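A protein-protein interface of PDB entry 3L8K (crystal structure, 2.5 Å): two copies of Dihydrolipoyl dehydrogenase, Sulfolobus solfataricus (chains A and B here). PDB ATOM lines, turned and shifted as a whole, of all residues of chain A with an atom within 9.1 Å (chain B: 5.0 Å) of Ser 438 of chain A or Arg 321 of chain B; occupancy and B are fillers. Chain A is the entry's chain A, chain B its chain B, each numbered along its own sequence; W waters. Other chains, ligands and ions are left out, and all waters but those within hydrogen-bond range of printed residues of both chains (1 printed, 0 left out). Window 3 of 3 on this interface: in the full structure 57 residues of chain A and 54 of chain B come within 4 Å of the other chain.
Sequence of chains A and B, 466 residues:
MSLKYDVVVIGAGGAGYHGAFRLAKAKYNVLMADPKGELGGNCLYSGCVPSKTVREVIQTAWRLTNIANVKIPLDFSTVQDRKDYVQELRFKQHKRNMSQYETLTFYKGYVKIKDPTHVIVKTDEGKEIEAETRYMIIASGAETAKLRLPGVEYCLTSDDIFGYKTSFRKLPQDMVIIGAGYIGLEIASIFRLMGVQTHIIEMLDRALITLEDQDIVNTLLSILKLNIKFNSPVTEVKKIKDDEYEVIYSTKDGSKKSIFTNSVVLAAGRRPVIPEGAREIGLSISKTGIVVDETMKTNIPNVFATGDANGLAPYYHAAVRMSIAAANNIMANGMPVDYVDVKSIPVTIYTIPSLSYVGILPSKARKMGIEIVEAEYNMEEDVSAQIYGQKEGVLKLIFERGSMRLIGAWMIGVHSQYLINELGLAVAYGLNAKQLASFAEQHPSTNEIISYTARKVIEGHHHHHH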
ATOM      1  N   ASN A 432     -26.405  -5.706  12.004  1.00  0.00           N
ATOM      2  CA  ASN A 432     -25.372  -5.738  10.958  1.00  0.00           C
ATOM      3  C   ASN A 432     -24.598  -4.414  10.907  1.00  0.00           C
ATOM      4  O   ASN A 432     -24.954  -3.439  11.589  1.00  0.00           O
ATOM      5  CB  ASN A 432     -25.968  -6.136   9.599  1.00  0.00           C
ATOM      6  CG  ASN A 432     -27.059  -5.166   9.097  1.00  0.00           C
ATOM      7  OD1 ASN A 432     -27.048  -3.951   9.406  1.00  0.00           O
ATOM      8  ND2 ASN A 432     -28.008  -5.701   8.329  1.00  0.00           N
ATOM      9  N   ALA A 433     -23.518  -4.384  10.141  1.00  0.00           N
ATOM     10  CA  ALA A 433     -22.678  -3.188  10.083  1.00  0.00           C
ATOM     11  C   ALA A 433     -23.500  -1.922   9.823  1.00  0.00           C
ATOM     12  O   ALA A 433     -23.270  -0.859  10.434  1.00  0.00           O
ATOM     13  CB  ALA A 433     -21.560  -3.366   9.051  1.00  0.00           C
ATOM     14  N   LYS A 434     -24.476  -2.045   8.928  1.00  0.00           N
ATOM     15  CA  LYS A 434     -25.322  -0.912   8.516  1.00  0.00           C
ATOM     16  C   LYS A 434     -26.133  -0.316   9.637  1.00  0.00           C
ATOM     17  O   LYS A 434     -26.253   0.905   9.761  1.00  0.00           O
ATOM     18  CB  LYS A 434     -26.312  -1.364   7.454  1.00  0.00           C
ATOM     19  CG  LYS A 434     -25.977  -0.891   6.084  1.00  0.00           C
ATOM     20  CD  LYS A 434     -24.686  -1.492   5.604  1.00  0.00           C
ATOM     21  CE  LYS A 434     -23.899  -0.532   4.669  1.00  0.00           C
ATOM     22  NZ  LYS A 434     -24.661  -0.101   3.444  1.00  0.00           N
ATOM     23  N   GLN A 435     -26.760  -1.193  10.398  1.00  0.00           N
ATOM     24  CA  GLN A 435     -27.492  -0.796  11.584  1.00  0.00           C
ATOM     25  C   GLN A 435     -26.597  -0.115  12.628  1.00  0.00           C
ATOM     26  O   GLN A 435     -27.002   0.869  13.243  1.00  0.00           O
ATOM     27  CB  GLN A 435     -28.208  -2.020  12.155  1.00  0.00           C
ATOM     28  CG  GLN A 435     -29.290  -2.548  11.174  1.00  0.00           C
ATOM     29  CD  GLN A 435     -29.934  -3.865  11.594  1.00  0.00           C
ATOM     30  OE1 GLN A 435     -29.269  -4.905  11.712  1.00  0.00           O
ATOM     31  NE2 GLN A 435     -31.240  -3.828  11.784  1.00  0.00           N
ATOM     32  N   LEU A 436     -25.376  -0.616  12.783  1.00  0.00           N
ATOM     33  CA  LEU A 436     -24.356  -0.010  13.679  1.00  0.00           C
ATOM     34  C   LEU A 436     -23.868   1.349  13.193  1.00  0.00           C
ATOM     35  O   LEU A 436     -23.772   2.314  13.984  1.00  0.00           O
ATOM     36  CB  LEU A 436     -23.161  -0.964  13.869  1.00  0.00           C
ATOM     37  CG  LEU A 436     -23.051  -1.720  15.209  1.00  0.00           C
ATOM     38  CD1 LEU A 436     -24.310  -2.411  15.543  1.00  0.00           C
ATOM     39  CD2 LEU A 436     -21.916  -2.731  15.189  1.00  0.00           C
ATOM     40  N   ALA A 437     -23.584   1.427  11.894  1.00  0.00           N
ATOM     41  CA  ALA A 437     -23.250   2.702  11.222  1.00  0.00           C
ATOM     42  C   ALA A 437     -24.376   3.735  11.389  1.00  0.00           C
ATOM     43  O   ALA A 437     -24.099   4.881  11.774  1.00  0.00           O
ATOM     44  CB  ALA A 437     -22.972   2.480   9.759  1.00  0.00           C
ATOM     45  N   SER A 438     -25.637   3.338  11.138  1.00  0.00           N
ATOM     46  CA  SER A 438     -26.760   4.297  11.193  1.00  0.00           C
ATOM     47  C   SER A 438     -27.140   4.768  12.587  1.00  0.00           C
ATOM     48  O   SER A 438     -27.878   5.737  12.714  1.00  0.00           O
ATOM     49  CB  SER A 438     -28.011   3.703  10.596  1.00  0.00           C
ATOM     50  OG  SER A 438     -27.817   3.518   9.232  1.00  0.00           O
ATOM     51  N   PHE A 439     -26.697   4.040  13.614  1.00  0.00           N
ATOM     52  CA  PHE A 439     -26.969   4.448  14.975  1.00  0.00           C
ATOM     53  C   PHE A 439     -25.981   5.575  15.364  1.00  0.00           C
ATOM     54  O   PHE A 439     -24.883   5.624  14.852  1.00  0.00           O
ATOM     55  CB  PHE A 439     -26.922   3.257  15.955  1.00  0.00           C
ATOM     56  CG  PHE A 439     -27.331   3.645  17.350  1.00  0.00           C
ATOM     57  CD1 PHE A 439     -28.597   4.158  17.585  1.00  0.00           C
ATOM     58  CD2 PHE A 439     -26.440   3.573  18.408  1.00  0.00           C
ATOM     59  CE1 PHE A 439     -28.980   4.579  18.854  1.00  0.00           C
ATOM     60  CE2 PHE A 439     -26.830   3.988  19.707  1.00  0.00           C
ATOM     61  CZ  PHE A 439     -28.084   4.494  19.926  1.00  0.00           C
ATOM     62  N   ALA A 440     -26.415   6.507  16.197  1.00  0.00           N
ATOM     63  CA  ALA A 440     -25.619   7.715  16.566  1.00  0.00           C
ATOM     64  C   ALA A 440     -25.474   7.786  18.065  1.00  0.00           C
ATOM     65  O   ALA A 440     -26.309   8.383  18.733  1.00  0.00           O
ATOM     66  CB  ALA A 440     -26.295   9.011  16.072  1.00  0.00           C
ATOM     67  N   GLU A 441     -24.424   7.163  18.576  1.00  0.00           N
ATOM     68  CA  GLU A 441     -24.134   7.186  20.001  1.00  0.00           C
ATOM     69  C   GLU A 441     -23.784   8.578  20.541  1.00  0.00           C
ATOM     70  O   GLU A 441     -23.118   9.406  19.896  1.00  0.00           O
ATOM     71  CB  GLU A 441     -22.973   6.253  20.355  1.00  0.00           C
ATOM     72  CG  GLU A 441     -23.197   4.775  20.049  1.00  0.00           C
ATOM     73  CD  GLU A 441     -22.636   4.401  18.704  1.00  0.00           C
ATOM     74  OE1 GLU A 441     -22.106   5.343  18.029  1.00  0.00           O
ATOM     75  OE2 GLU A 441     -22.743   3.187  18.321  1.00  0.00           O
ATOM     76  N   ILE A 450     -17.930   3.041  18.326  1.00  0.00           N
ATOM     77  CA  ILE A 450     -18.594   1.888  17.699  1.00  0.00           C
ATOM     78  C   ILE A 450     -19.253   2.237  16.327  1.00  0.00           C
ATOM     79  O   ILE A 450     -18.873   1.638  15.301  1.00  0.00           O
ATOM     80  CB  ILE A 450     -19.660   1.259  18.633  1.00  0.00           C
ATOM     81  CG1 ILE A 450     -18.959   0.626  19.819  1.00  0.00           C
ATOM     82  CG2 ILE A 450     -20.504   0.259  17.868  1.00  0.00           C
ATOM     83  CD1 ILE A 450     -19.801   0.481  21.081  1.00  0.00           C
ATOM     84  N   SER A 451     -20.213   3.178  16.291  1.00  0.00           N
ATOM     85  CA  SER A 451     -20.788   3.592  14.981  1.00  0.00           C
ATOM     86  C   SER A 451     -19.683   4.108  14.060  1.00  0.00           C
ATOM     87  O   SER A 451     -19.602   3.725  12.883  1.00  0.00           O
ATOM     88  CB  SER A 451     -21.921   4.609  15.106  1.00  0.00           C
ATOM     89  OG  SER A 451     -21.528   5.806  15.749  1.00  0.00           O
ATOM     90  N   TYR A 452     -18.781   4.903  14.623  1.00  0.00           N
ATOM     91  CA  TYR A 452     -17.580   5.302  13.915  1.00  0.00           C
ATOM     92  C   TYR A 452     -16.814   4.108  13.257  1.00  0.00           C
ATOM     93  O   TYR A 452     -16.529   4.151  12.062  1.00  0.00           O
ATOM     94  CB  TYR A 452     -16.657   6.082  14.845  1.00  0.00           C
ATOM     95  CG  TYR A 452     -15.495   6.670  14.107  1.00  0.00           C
ATOM     96  CD1 TYR A 452     -15.543   7.978  13.639  1.00  0.00           C
ATOM     97  CD2 TYR A 452     -14.351   5.908  13.845  1.00  0.00           C
ATOM     98  CE1 TYR A 452     -14.487   8.521  12.945  1.00  0.00           C
ATOM     99  CE2 TYR A 452     -13.283   6.442  13.161  1.00  0.00           C
ATOM    100  CZ  TYR A 452     -13.357   7.746  12.702  1.00  0.00           C
ATOM    101  OH  TYR A 452     -12.304   8.293  12.013  1.00  0.00           O
ATOM    102  N   ALA A 454     -17.961   1.094  12.638  1.00  0.00           N
ATOM    103  CA  ALA A 454     -18.868   0.463  11.675  1.00  0.00           C
ATOM    104  C   ALA A 454     -18.936   1.282  10.363  1.00  0.00           C
ATOM    105  O   ALA A 454     -18.996   0.705   9.300  1.00  0.00           O
ATOM    106  CB  ALA A 454     -20.246   0.269  12.276  1.00  0.00           C
ATOM    107  N   ARG A 455     -18.916   2.613  10.454  1.00  0.00           N
ATOM    108  CA  ARG A 455     -18.870   3.475   9.248  1.00  0.00           C
ATOM    109  C   ARG A 455     -17.612   3.198   8.400  1.00  0.00           C
ATOM    110  O   ARG A 455     -17.661   3.242   7.178  1.00  0.00           O
ATOM    111  CB  ARG A 455     -18.950   4.953   9.631  1.00  0.00           C
ATOM    112  CG  ARG A 455     -20.312   5.351  10.103  1.00  0.00           C
ATOM    113  CD  ARG A 455     -20.366   6.637  10.872  1.00  0.00           C
ATOM    114  NE  ARG A 455     -21.666   6.765  11.550  1.00  0.00           N
ATOM    115  CZ  ARG A 455     -21.949   7.607  12.548  1.00  0.00           C
ATOM    116  NH1 ARG A 455     -21.036   8.461  12.972  1.00  0.00           N
ATOM    117  NH2 ARG A 455     -23.154   7.604  13.128  1.00  0.00           N
ATOM    118  N   ILE A 458     -17.521  -0.032   5.765  1.00  0.00           N
ATOM    119  CA  ILE A 458     -18.287   0.206   4.535  1.00  0.00           C
ATOM    120  C   ILE A 458     -17.422   1.045   3.635  1.00  0.00           C
ATOM    121  O   ILE A 458     -17.058   0.603   2.559  1.00  0.00           O
ATOM    122  CB  ILE A 458     -19.659   0.912   4.819  1.00  0.00           C
ATOM    123  CG1 ILE A 458     -20.572  -0.008   5.668  1.00  0.00           C
ATOM    124  CG2 ILE A 458     -20.346   1.349   3.501  1.00  0.00           C
ATOM    125  CD1 ILE A 458     -21.007   0.571   7.019  1.00  0.00           C
ATOM    126  N   HIS B 317     -23.384  14.434  17.723  1.00  0.00           N
ATOM    127  CA  HIS B 317     -23.571  13.076  17.186  1.00  0.00           C
ATOM    128  C   HIS B 317     -24.741  13.001  16.220  1.00  0.00           C
ATOM    129  O   HIS B 317     -24.732  12.193  15.316  1.00  0.00           O
ATOM    130  CB  HIS B 317     -23.721  12.015  18.310  1.00  0.00           C
ATOM    131  CG  HIS B 317     -24.800  12.313  19.309  1.00  0.00           C
ATOM    132  ND1 HIS B 317     -24.739  13.379  20.191  1.00  0.00           N
ATOM    133  CD2 HIS B 317     -25.956  11.659  19.594  1.00  0.00           C
ATOM    134  CE1 HIS B 317     -25.818  13.375  20.958  1.00  0.00           C
ATOM    135  NE2 HIS B 317     -26.564  12.334  20.625  1.00  0.00           N
ATOM    136  N   ALA B 318     -25.764  13.819  16.427  1.00  0.00           N
ATOM    137  CA  ALA B 318     -26.808  13.940  15.411  1.00  0.00           C
ATOM    138  C   ALA B 318     -26.235  14.583  14.149  1.00  0.00           C
ATOM    139  O   ALA B 318     -26.585  14.199  13.029  1.00  0.00           O
ATOM    140  CB  ALA B 318     -27.952  14.750  15.909  1.00  0.00           C
ATOM    141  N   ALA B 319     -25.410  15.602  14.352  1.00  0.00           N
ATOM    142  CA  ALA B 319     -24.753  16.290  13.257  1.00  0.00           C
ATOM    143  C   ALA B 319     -23.911  15.326  12.408  1.00  0.00           C
ATOM    144  O   ALA B 319     -24.014  15.333  11.169  1.00  0.00           O
ATOM    145  CB  ALA B 319     -23.916  17.464  13.793  1.00  0.00           C
ATOM    146  N   VAL B 320     -23.131  14.461  13.047  1.00  0.00           N
ATOM    147  CA  VAL B 320     -22.292  13.511  12.315  1.00  0.00           C
ATOM    148  C   VAL B 320     -23.175  12.585  11.453  1.00  0.00           C
ATOM    149  O   VAL B 320     -22.955  12.413  10.256  1.00  0.00           O
ATOM    150  CB  VAL B 320     -21.382  12.689  13.286  1.00  0.00           C
ATOM    151  CG1 VAL B 320     -20.651  11.522  12.566  1.00  0.00           C
ATOM    152  CG2 VAL B 320     -20.353  13.588  13.993  1.00  0.00           C
ATOM    153  N   ARG B 321     -24.188  11.993  12.073  1.00  0.00           N
ATOM    154  CA  ARG B 321     -25.132  11.169  11.366  1.00  0.00           C
ATOM    155  C   ARG B 321     -25.783  11.873  10.144  1.00  0.00           C
ATOM    156  O   ARG B 321     -25.876  11.271   9.081  1.00  0.00           O
ATOM    157  CB  ARG B 321     -26.207  10.659  12.345  1.00  0.00           C
ATOM    158  CG  ARG B 321     -27.219   9.721  11.751  1.00  0.00           C
ATOM    159  CD  ARG B 321     -26.577   8.490  11.153  1.00  0.00           C
ATOM    160  NE  ARG B 321     -27.617   7.691  10.515  1.00  0.00           N
ATOM    161  CZ  ARG B 321     -27.778   7.522   9.207  1.00  0.00           C
ATOM    162  NH1 ARG B 321     -26.917   8.033   8.318  1.00  0.00           N
ATOM    163  NH2 ARG B 321     -28.807   6.819   8.784  1.00  0.00           N
ATOM    164  N   MET B 322     -26.219  13.120  10.289  1.00  0.00           N
ATOM    165  CA  MET B 322     -26.799  13.887   9.145  1.00  0.00           C
ATOM    166  C   MET B 322     -25.751  14.107   8.051  1.00  0.00           C
ATOM    167  O   MET B 322     -26.036  13.972   6.889  1.00  0.00           O
ATOM    168  CB  MET B 322     -27.397  15.236   9.582  1.00  0.00           C
ATOM    169  CG  MET B 322     -28.499  15.184  10.688  1.00  0.00           C
ATOM    170  SD  MET B 322     -29.050  16.737  11.401  1.00  0.00           S
ATOM    171  CE  MET B 322     -28.386  16.724  12.980  1.00  0.00           C
ATOM    172  N   SER B 323     -24.502  14.388   8.439  1.00  0.00           N
ATOM    173  CA  SER B 323     -23.403  14.585   7.476  1.00  0.00           C
ATOM    174  C   SER B 323     -23.230  13.332   6.646  1.00  0.00           C
ATOM    175  O   SER B 323     -23.060  13.392   5.442  1.00  0.00           O
ATOM    176  CB  SER B 323     -22.085  14.903   8.216  1.00  0.00           C
ATOM    177  OG  SER B 323     -21.124  15.559   7.387  1.00  0.00           O
ATOM    178  N   ILE B 324     -23.235  12.187   7.312  1.00  0.00           N
ATOM    179  CA  ILE B 324     -23.053  10.913   6.618  1.00  0.00           C
ATOM    180  C   ILE B 324     -24.239  10.684   5.682  1.00  0.00           C
ATOM    181  O   ILE B 324     -24.056  10.294   4.528  1.00  0.00           O
ATOM    182  CB  ILE B 324     -22.960   9.742   7.591  1.00  0.00           C
ATOM    183  CG1 ILE B 324     -21.666   9.823   8.426  1.00  0.00           C
ATOM    184  CG2 ILE B 324     -23.046   8.389   6.833  1.00  0.00           C
ATOM    185  CD1 ILE B 324     -20.336   9.760   7.601  1.00  0.00           C
ATOM    186  N   ALA B 325     -25.448  10.983   6.151  1.00  0.00           N
ATOM    187  CA  ALA B 325     -26.630  10.794   5.302  1.00  0.00           C
ATOM    188  C   ALA B 325     -26.607  11.681   4.042  1.00  0.00           C
ATOM    189  O   ALA B 325     -26.933  11.227   2.989  1.00  0.00           O
ATOM    190  CB  ALA B 325     -27.896  11.037   6.097  1.00  0.00           C
ATOM    191  N   ASP B 338     -30.603   7.259   2.008  1.00  0.00           N
ATOM    192  CA  ASP B 338     -30.318   7.299   3.443  1.00  0.00           C
ATOM    193  C   ASP B 338     -31.142   8.412   4.138  1.00  0.00           C
ATOM    194  O   ASP B 338     -31.406   9.455   3.578  1.00  0.00           O
ATOM    195  CB  ASP B 338     -28.792   7.446   3.660  1.00  0.00           C
ATOM    196  CG  ASP B 338     -28.320   7.026   5.070  1.00  0.00           C
ATOM    197  OD1 ASP B 338     -29.148   6.532   5.869  1.00  0.00           O
ATOM    198  OD2 ASP B 338     -27.118   7.181   5.395  1.00  0.00           O
ATOM    199  N   TYR B 339     -31.531   8.138   5.366  1.00  0.00           N
ATOM    200  CA  TYR B 339     -32.534   8.898   6.115  1.00  0.00           C
ATOM    201  C   TYR B 339     -32.110   8.945   7.579  1.00  0.00           C
ATOM    202  O   TYR B 339     -31.611   7.961   8.084  1.00  0.00           O
ATOM    203  CB  TYR B 339     -33.896   8.167   6.094  1.00  0.00           C
ATOM    204  CG  TYR B 339     -34.540   7.894   4.743  1.00  0.00           C
ATOM    205  CD1 TYR B 339     -35.682   8.600   4.336  1.00  0.00           C
ATOM    206  CD2 TYR B 339     -34.046   6.906   3.894  1.00  0.00           C
ATOM    207  CE1 TYR B 339     -36.288   8.352   3.115  1.00  0.00           C
ATOM    208  CE2 TYR B 339     -34.652   6.647   2.664  1.00  0.00           C
ATOM    209  CZ  TYR B 339     -35.771   7.380   2.284  1.00  0.00           C
ATOM    210  OH  TYR B 339     -36.385   7.140   1.075  1.00  0.00           O
ATOM    211  N   VAL B 340     -32.410  10.025   8.267  1.00  0.00           N
ATOM    212  CA  VAL B 340     -32.097  10.122   9.656  1.00  0.00           C
ATOM    213  C   VAL B 340     -33.374  10.050  10.497  1.00  0.00           C
ATOM    214  O   VAL B 340     -34.319  10.842  10.312  1.00  0.00           O
ATOM    215  CB  VAL B 340     -31.340  11.435   9.893  1.00  0.00           C
ATOM    216  CG1 VAL B 340     -31.097  11.700  11.380  1.00  0.00           C
ATOM    217  CG2 VAL B 340     -30.035  11.415   9.085  1.00  0.00           C
ATOM    218  N   ILE B 345     -32.116   9.197  18.207  1.00  0.00           N
ATOM    219  CA  ILE B 345     -30.826   9.711  18.626  1.00  0.00           C
ATOM    220  C   ILE B 345     -30.848  10.120  20.093  1.00  0.00           C
ATOM    221  O   ILE B 345     -31.603  10.989  20.462  1.00  0.00           O
ATOM    222  CB  ILE B 345     -30.344  10.847  17.727  1.00  0.00           C
ATOM    223  CG1 ILE B 345     -30.208  10.303  16.291  1.00  0.00           C
ATOM    224  CG2 ILE B 345     -29.015  11.375  18.234  1.00  0.00           C
ATOM    225  CD1 ILE B 345     -30.234  11.388  15.218  1.00  0.00           C
ATOM    226  N   TYR B 429     -33.892  -0.178  16.857  1.00  0.00           N
ATOM    227  CA  TYR B 429     -34.163  -1.387  16.080  1.00  0.00           C
ATOM    228  C   TYR B 429     -35.235  -2.250  16.728  1.00  0.00           C
ATOM    229  O   TYR B 429     -35.413  -3.395  16.372  1.00  0.00           O
ATOM    230  CB  TYR B 429     -32.856  -2.144  15.732  1.00  0.00           C
ATOM    231  CG  TYR B 429     -31.927  -1.244  14.954  1.00  0.00           C
ATOM    232  CD1 TYR B 429     -32.291  -0.767  13.686  1.00  0.00           C
ATOM    233  CD2 TYR B 429     -30.738  -0.762  15.522  1.00  0.00           C
ATOM    234  CE1 TYR B 429     -31.454   0.128  12.975  1.00  0.00           C
ATOM    235  CE2 TYR B 429     -29.898   0.116  14.823  1.00  0.00           C
ATOM    236  CZ  TYR B 429     -30.270   0.567  13.553  1.00  0.00           C
ATOM    237  OH  TYR B 429     -29.446   1.443  12.847  1.00  0.00           O
HETATM  238  O   HOH W   1     -23.089   9.913  14.870  1.00  0.00           O
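No position is printed for both chains.
Arg 321 of chain B touches just one residue of chain A: Ser 438 (3.0 Å). Of chain A, only Arg 455 comes within 4 Å of Val 320 of chain B. Of the printed residues of chain B, Phe 439 of chain A touches Tyr 429 (3.9 Å). Of the printed residues of chain B, Arg 455 of chain A touches Val 320. Of the printed residues of chain A, Tyr 429 of chain B touches Gln 435 (2.5 Å), Ser 438 (3.5 Å) and Phe 439 (3.9 Å). The nearest printed residue of chain A that does not touch Arg 321 of chain B is Arg 455 of chain A (4.1 Å). The nearest printed residue of chain B that does not touch Arg 455 of chain A is Arg 321 of chain B (4.1 Å).
Among the printed residues, merely in contact across the chains: Ser 438 of chain A with Tyr 429 of chain B (3.5 Å), Phe 439 of chain A with Tyr 429 of chain B (3.9 Å), Ala 440 of chain A with His 317 of chain B (3.4 Å), Glu 441 of chain A with His 317 of chain B (3.1 Å) and Arg 455 of chain A with Val 320 of chain B (3.1 Å).
The backbone carbonyl oxygen of Ser 438 of chain A is in hydrogen-bond range of the guanidinium group of Arg 321 of chain B, 3.0 Å away. O of Gln 435 of chain A sits at hydrogen-bond distance from OH of Tyr 429 of chain B, 2.5 Å away.
Printed residues of chain B that touch a printed residue of chain A: His 317, Val 320, Arg 321 and Tyr 429. Hydrophobic or aromatic side chains of chain B within 4 Å of the printed part of chain A: His 317, Val 320 and Tyr 429. Along chain B the printed residues that touch a printed residue of chain A span positions 317 to 429. Hydrophobic or aromatic side chains of chain A that line the printed part of chain B: Ala 440. Along chain A the printed residues that touch a printed residue of chain B span positions 435 to 455. Among the printed residues, no Asp or Glu carboxylate lies within 4 Å of a Lys or Arg side-chain nitrogen of the other chain.
Water W1 lies within hydrogen-bond range of the backbone carbonyl oxygen of His 317 of chain B (2.8 Å) and the guanidinium group of Arg 455 of chain A (2.9 Å).
NH2 of Arg 321 of chain B is in salt-bridge range of OD1 of Asp 338 of chain B, at 2.9 Å. O of Ala 437 of chain A lies within hydrogen-bond range of NE of Arg 455 of chain A (3.1 Å). The backbone carbonyl oxygen (O) of Lys 434 of chain A lies within hydrogen-bond range of the side-chain hydroxyl (OG) of Ser 438 of chain A (3.1 Å). The backbone NH of Gln 435 of chain A lies within hydrogen-bond range of the side-chain amide oxygen of Asn 432 of chain A (2.9 Å). The backbone carbonyl oxygen (O) of Phe 439 of chain A sits close to the side-chain hydroxyl (OG) of Ser 451 of chain A, 3.5 Å away. The guanidinium group of Arg 321 of chain B is in hydrogen-bond range of the backbone carbonyl oxygen of Tyr 339 of chain B (3.1 Å).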
